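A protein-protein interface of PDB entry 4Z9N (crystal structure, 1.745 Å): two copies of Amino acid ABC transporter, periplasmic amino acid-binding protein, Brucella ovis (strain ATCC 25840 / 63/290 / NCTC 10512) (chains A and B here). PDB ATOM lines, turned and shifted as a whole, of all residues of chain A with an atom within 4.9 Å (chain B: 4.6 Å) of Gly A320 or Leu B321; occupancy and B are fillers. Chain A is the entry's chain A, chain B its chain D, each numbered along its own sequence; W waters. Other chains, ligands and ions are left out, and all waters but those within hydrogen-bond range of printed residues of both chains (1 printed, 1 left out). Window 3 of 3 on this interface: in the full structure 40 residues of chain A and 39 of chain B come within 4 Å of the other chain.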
ATOM      1  N   GLY A 311      -9.834 -20.767  19.844  1.00  0.00           N
ATOM      2  CA  GLY A 311      -9.611 -21.085  21.250  1.00  0.00           C
ATOM      3  C   GLY A 311      -8.152 -21.309  21.611  1.00  0.00           C
ATOM      4  O   GLY A 311      -7.310 -20.462  21.341  1.00  0.00           O
ATOM      5  N   LEU A 312      -7.860 -22.461  22.222  1.00  0.00           N
ATOM      6  CA  LEU A 312      -6.497 -22.833  22.590  1.00  0.00           C
ATOM      7  C   LEU A 312      -5.568 -22.899  21.396  1.00  0.00           C
ATOM      8  O   LEU A 312      -4.345 -22.827  21.556  1.00  0.00           O
ATOM      9  CB  LEU A 312      -6.469 -24.203  23.281  1.00  0.00           C
ATOM     10  CG  LEU A 312      -7.089 -24.376  24.663  1.00  0.00           C
ATOM     11  CD1 LEU A 312      -6.880 -25.827  25.116  1.00  0.00           C
ATOM     12  CD2 LEU A 312      -6.480 -23.394  25.661  1.00  0.00           C
ATOM     13  N   ALA A 314      -5.536 -20.802  18.909  1.00  0.00           N
ATOM     14  CA  ALA A 314      -5.106 -19.481  18.419  1.00  0.00           C
ATOM     15  C   ALA A 314      -3.587 -19.337  18.526  1.00  0.00           C
ATOM     16  O   ALA A 314      -2.916 -20.063  19.263  1.00  0.00           O
ATOM     17  CB  ALA A 314      -5.790 -18.360  19.215  1.00  0.00           C
ATOM     18  N   GLN A 315      -3.044 -18.378  17.789  1.00  0.00           N
ATOM     19  CA  GLN A 315      -1.643 -18.006  17.957  1.00  0.00           C
ATOM     20  C   GLN A 315      -1.344 -17.586  19.393  1.00  0.00           C
ATOM     21  O   GLN A 315      -2.203 -17.034  20.073  1.00  0.00           O
ATOM     22  CB  GLN A 315      -1.288 -16.863  17.008  1.00  0.00           C
ATOM     23  CG  GLN A 315      -1.173 -17.324  15.560  1.00  0.00           C
ATOM     24  CD  GLN A 315       0.163 -17.996  15.261  1.00  0.00           C
ATOM     25  OE1 GLN A 315       1.181 -17.694  15.889  1.00  0.00           O
ATOM     26  NE2 GLN A 315       0.162 -18.919  14.305  1.00  0.00           N
ATOM     27  N   TRP A 316      -0.111 -17.840  19.822  1.00  0.00           N
ATOM     28  CA  TRP A 316       0.358 -17.525  21.170  1.00  0.00           C
ATOM     29  C   TRP A 316       0.183 -16.063  21.524  1.00  0.00           C
ATOM     30  O   TRP A 316      -0.068 -15.732  22.671  1.00  0.00           O
ATOM     31  CB  TRP A 316       1.843 -17.893  21.306  1.00  0.00           C
ATOM     32  CG  TRP A 316       2.698 -17.074  20.377  1.00  0.00           C
ATOM     33  CD1 TRP A 316       2.890 -17.276  19.041  1.00  0.00           C
ATOM     34  CD2 TRP A 316       3.453 -15.907  20.721  1.00  0.00           C
ATOM     35  NE1 TRP A 316       3.742 -16.308  18.527  1.00  0.00           N
ATOM     36  CE2 TRP A 316       4.097 -15.457  19.542  1.00  0.00           C
ATOM     37  CE3 TRP A 316       3.666 -15.209  21.915  1.00  0.00           C
ATOM     38  CZ2 TRP A 316       4.937 -14.341  19.528  1.00  0.00           C
ATOM     39  CZ3 TRP A 316       4.492 -14.085  21.898  1.00  0.00           C
ATOM     40  CH2 TRP A 316       5.116 -13.665  20.708  1.00  0.00           C
ATOM     41  N   LYS A 318      -2.136 -14.163  20.445  1.00  0.00           N
ATOM     42  CA  LYS A 318      -3.552 -13.810  20.408  1.00  0.00           C
ATOM     43  C   LYS A 318      -4.350 -14.663  21.381  1.00  0.00           C
ATOM     44  O   LYS A 318      -5.520 -14.944  21.146  1.00  0.00           O
ATOM     45  CB  LYS A 318      -4.097 -13.960  18.999  1.00  0.00           C
ATOM     46  CG  LYS A 318      -3.532 -12.900  18.073  1.00  0.00           C
ATOM     47  CD  LYS A 318      -4.075 -13.027  16.674  1.00  0.00           C
ATOM     48  CE  LYS A 318      -3.770 -11.757  15.900  1.00  0.00           C
ATOM     49  NZ  LYS A 318      -4.214 -11.895  14.498  1.00  0.00           N
ATOM     50  N   GLY A 319      -3.692 -15.116  22.445  1.00  0.00           N
ATOM     51  CA  GLY A 319      -4.377 -15.790  23.532  1.00  0.00           C
ATOM     52  C   GLY A 319      -4.315 -17.301  23.498  1.00  0.00           C
ATOM     53  O   GLY A 319      -4.713 -17.953  24.469  1.00  0.00           O
ATOM     54  N   GLY A 320      -3.798 -17.856  22.400  1.00  0.00           N
ATOM     55  CA  GLY A 320      -3.718 -19.297  22.231  1.00  0.00           C
ATOM     56  C   GLY A 320      -2.407 -19.913  22.705  1.00  0.00           C
ATOM     57  O   GLY A 320      -1.577 -19.240  23.340  1.00  0.00           O
ATOM     58  N   LEU A 321      -2.230 -21.196  22.396  1.00  0.00           N
ATOM     59  CA  LEU A 321      -1.054 -21.958  22.810  1.00  0.00           C
ATOM     60  C   LEU A 321      -0.138 -22.256  21.650  1.00  0.00           C
ATOM     61  O   LEU A 321       0.965 -22.784  21.853  1.00  0.00           O
ATOM     62  CB  LEU A 321      -1.462 -23.282  23.466  1.00  0.00           C
ATOM     63  CG  LEU A 321      -2.360 -23.191  24.694  1.00  0.00           C
ATOM     64  CD1 LEU A 321      -2.639 -24.607  25.219  1.00  0.00           C
ATOM     65  CD2 LEU A 321      -1.699 -22.295  25.772  1.00  0.00           C
ATOM     66  N   GLN A 322      -0.577 -21.949  20.426  1.00  0.00           N
ATOM     67  CA  GLN A 322       0.215 -22.318  19.249  1.00  0.00           C
ATOM     68  C   GLN A 322       1.368 -21.332  19.033  1.00  0.00           C
ATOM     69  O   GLN A 322       1.156 -20.167  18.713  1.00  0.00           O
ATOM     70  CB  GLN A 322      -0.677 -22.390  18.010  1.00  0.00           C
ATOM     71  CG  GLN A 322      -1.631 -23.608  18.023  1.00  0.00           C
ATOM     72  CD  GLN A 322      -0.898 -24.940  17.830  1.00  0.00           C
ATOM     73  OE1 GLN A 322       0.305 -24.971  17.600  1.00  0.00           O
ATOM     74  NE2 GLN A 322      -1.625 -26.042  17.938  1.00  0.00           N
ATOM     75  N   TYR A 323       2.589 -21.832  19.180  1.00  0.00           N
ATOM     76  CA  TYR A 323       3.764 -20.969  19.254  1.00  0.00           C
ATOM     77  C   TYR A 323       4.785 -21.473  18.252  1.00  0.00           C
ATOM     78  O   TYR A 323       5.379 -22.537  18.451  1.00  0.00           O
ATOM     79  CB  TYR A 323       4.346 -20.984  20.678  1.00  0.00           C
ATOM     80  CG  TYR A 323       5.581 -20.112  20.894  1.00  0.00           C
ATOM     81  CD1 TYR A 323       6.867 -20.578  20.589  1.00  0.00           C
ATOM     82  CD2 TYR A 323       5.467 -18.851  21.461  1.00  0.00           C
ATOM     83  CE1 TYR A 323       8.000 -19.784  20.823  1.00  0.00           C
ATOM     84  CE2 TYR A 323       6.577 -18.064  21.687  1.00  0.00           C
ATOM     85  CZ  TYR A 323       7.843 -18.534  21.371  1.00  0.00           C
ATOM     86  OH  TYR A 323       8.952 -17.732  21.618  1.00  0.00           O
ATOM     87  N   TYR B 109       9.718 -19.077  27.993  1.00  0.00           N
ATOM     88  CA  TYR B 109       9.523 -18.306  26.760  1.00  0.00           C
ATOM     89  C   TYR B 109       9.968 -16.877  26.997  1.00  0.00           C
ATOM     90  O   TYR B 109       9.422 -16.213  27.856  1.00  0.00           O
ATOM     91  CB  TYR B 109       8.063 -18.309  26.313  1.00  0.00           C
ATOM     92  CG  TYR B 109       7.527 -19.676  25.942  1.00  0.00           C
ATOM     93  CD1 TYR B 109       7.008 -20.514  26.914  1.00  0.00           C
ATOM     94  CD2 TYR B 109       7.551 -20.125  24.629  1.00  0.00           C
ATOM     95  CE1 TYR B 109       6.513 -21.768  26.591  1.00  0.00           C
ATOM     96  CE2 TYR B 109       7.062 -21.377  24.293  1.00  0.00           C
ATOM     97  CZ  TYR B 109       6.550 -22.192  25.283  1.00  0.00           C
ATOM     98  OH  TYR B 109       6.051 -23.433  24.956  1.00  0.00           O
ATOM     99  N   LEU B 312       4.017 -15.018  29.753  1.00  0.00           N
ATOM    100  CA  LEU B 312       3.940 -16.153  28.833  1.00  0.00           C
ATOM    101  C   LEU B 312       4.199 -17.458  29.550  1.00  0.00           C
ATOM    102  O   LEU B 312       3.829 -18.519  29.056  1.00  0.00           O
ATOM    103  CB  LEU B 312       4.954 -16.005  27.696  1.00  0.00           C
ATOM    104  CG  LEU B 312       4.756 -14.828  26.756  1.00  0.00           C
ATOM    105  CD1 LEU B 312       5.913 -14.810  25.732  1.00  0.00           C
ATOM    106  CD2 LEU B 312       3.405 -14.944  26.078  1.00  0.00           C
ATOM    107  N   ALA B 314       3.120 -18.273  32.514  1.00  0.00           N
ATOM    108  CA  ALA B 314       2.013 -18.737  33.331  1.00  0.00           C
ATOM    109  C   ALA B 314       1.518 -20.060  32.759  1.00  0.00           C
ATOM    110  O   ALA B 314       1.761 -20.384  31.597  1.00  0.00           O
ATOM    111  CB  ALA B 314       0.864 -17.706  33.377  1.00  0.00           C
ATOM    112  N   GLY B 320      -1.209 -18.284  30.162  1.00  0.00           N
ATOM    113  CA  GLY B 320       0.123 -18.415  29.614  1.00  0.00           C
ATOM    114  C   GLY B 320       0.271 -19.507  28.572  1.00  0.00           C
ATOM    115  O   GLY B 320      -0.723 -20.004  28.041  1.00  0.00           O
ATOM    116  N   LEU B 321       1.518 -19.880  28.299  1.00  0.00           N
ATOM    117  CA  LEU B 321       1.852 -20.872  27.269  1.00  0.00           C
ATOM    118  C   LEU B 321       2.331 -22.208  27.837  1.00  0.00           C
ATOM    119  O   LEU B 321       2.527 -23.180  27.083  1.00  0.00           O
ATOM    120  CB  LEU B 321       2.948 -20.319  26.343  1.00  0.00           C
ATOM    121  CG  LEU B 321       2.656 -19.012  25.615  1.00  0.00           C
ATOM    122  CD1 LEU B 321       3.848 -18.601  24.729  1.00  0.00           C
ATOM    123  CD2 LEU B 321       1.376 -19.153  24.762  1.00  0.00           C
ATOM    124  N   GLN B 322       2.543 -22.283  29.150  1.00  0.00           N
ATOM    125  CA  GLN B 322       3.202 -23.473  29.686  1.00  0.00           C
ATOM    126  C   GLN B 322       2.196 -24.579  29.890  1.00  0.00           C
ATOM    127  O   GLN B 322       1.272 -24.469  30.706  1.00  0.00           O
ATOM    128  CB  GLN B 322       3.957 -23.168  30.991  1.00  0.00           C
ATOM    129  CG  GLN B 322       5.207 -22.308  30.795  1.00  0.00           C
ATOM    130  CD  GLN B 322       6.377 -23.098  30.215  1.00  0.00           C
ATOM    131  OE1 GLN B 322       6.272 -24.299  29.963  1.00  0.00           O
ATOM    132  NE2 GLN B 322       7.491 -22.417  29.985  1.00  0.00           N
ATOM    133  N   TYR B 323       2.383 -25.656  29.137  1.00  0.00           N
ATOM    134  CA  TYR B 323       1.376 -26.718  29.058  1.00  0.00           C
ATOM    135  C   TYR B 323       2.005 -28.060  29.367  1.00  0.00           C
ATOM    136  O   TYR B 323       2.822 -28.553  28.604  1.00  0.00           O
ATOM    137  CB  TYR B 323       0.749 -26.711  27.663  1.00  0.00           C
ATOM    138  CG  TYR B 323      -0.368 -27.706  27.381  1.00  0.00           C
ATOM    139  CD1 TYR B 323      -0.074 -28.993  26.923  1.00  0.00           C
ATOM    140  CD2 TYR B 323      -1.712 -27.329  27.479  1.00  0.00           C
ATOM    141  CE1 TYR B 323      -1.087 -29.892  26.625  1.00  0.00           C
ATOM    142  CE2 TYR B 323      -2.739 -28.227  27.162  1.00  0.00           C
ATOM    143  CZ  TYR B 323      -2.412 -29.499  26.740  1.00  0.00           C
ATOM    144  OH  TYR B 323      -3.410 -30.380  26.412  1.00  0.00           O
HETATM  145  O   HOH W   1       2.431 -23.806  24.196  1.00  0.00           O
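N of Leu B321 lies within hydrogen-bond range of O of Ala B314 (3.3 Å). The backbone NH of Leu A321 sits at hydrogen-bond distance from the backbone carbonyl oxygen of Leu A312 (2.8 Å). The backbone carbonyl oxygen (O) of Gln A315 sits at hydrogen-bond distance from the backbone NH (N) of Gly A320 (2.9 Å). The backbone NH (N) of Leu A321 lies within hydrogen-bond range of the backbone carbonyl oxygen (O) of Ala A314 (3.4 Å). The backbone carbonyl oxygen (O) of Leu B312 sits at hydrogen-bond distance from the backbone NH (N) of Leu B321 (2.8 Å). N of Trp A316 is in hydrogen-bond range of O of Gln A322 (2.9 Å).
Among the printed residues, pairs that only touch across the chains: Trp A316 with Leu B321 (3.7 Å), Gly A320 with Leu B321 (3.3 Å), Leu A321 with Gly B320 (3.4 Å), Leu A321 with Tyr B323 (3.7 Å), Tyr A323 with Tyr B109 (3.6 Å) and Tyr A323 with Leu B321 (3.7 Å).
Gly A311 touches none of the printed residues of chain B. Of chain B, only Leu B321 comes within 4 Å of Gly A320. Printed residues of chain A within 4 Å of Tyr B109: Tyr A323 (3.6 Å). Of chain A, only Trp A316 (3.7 Å), Gly A320 (3.3 Å) and Tyr A323 (3.7 Å) come within 4 Å of Leu B321. Of the printed residues of chain A, Tyr B323 touches Leu A321 (3.7 Å). The nearest residue of chain A that does not touch Leu B321 is Leu A321 (4.1 Å).
Of the 11 printed residues of chain A, 4 touch a printed residue of chain B. Among the printed residues, 6 pairs touch across the chains. Among the printed residues, no Asp or Glu carboxylate lies within 4 Å of a Lys or Arg side-chain nitrogen of the other chain.
Gly A320 touches Leu B321, and with the chains exchanged Leu A321 touches Gly B320. Leu A321 touches Tyr B323, and with the chains exchanged Tyr A323 touches Leu B321. 6 positions are printed for both chains.
Water W1 bridges the backbone carbonyl oxygen (O) of Leu A321 and the backbone carbonyl oxygen (O) of Leu B321.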
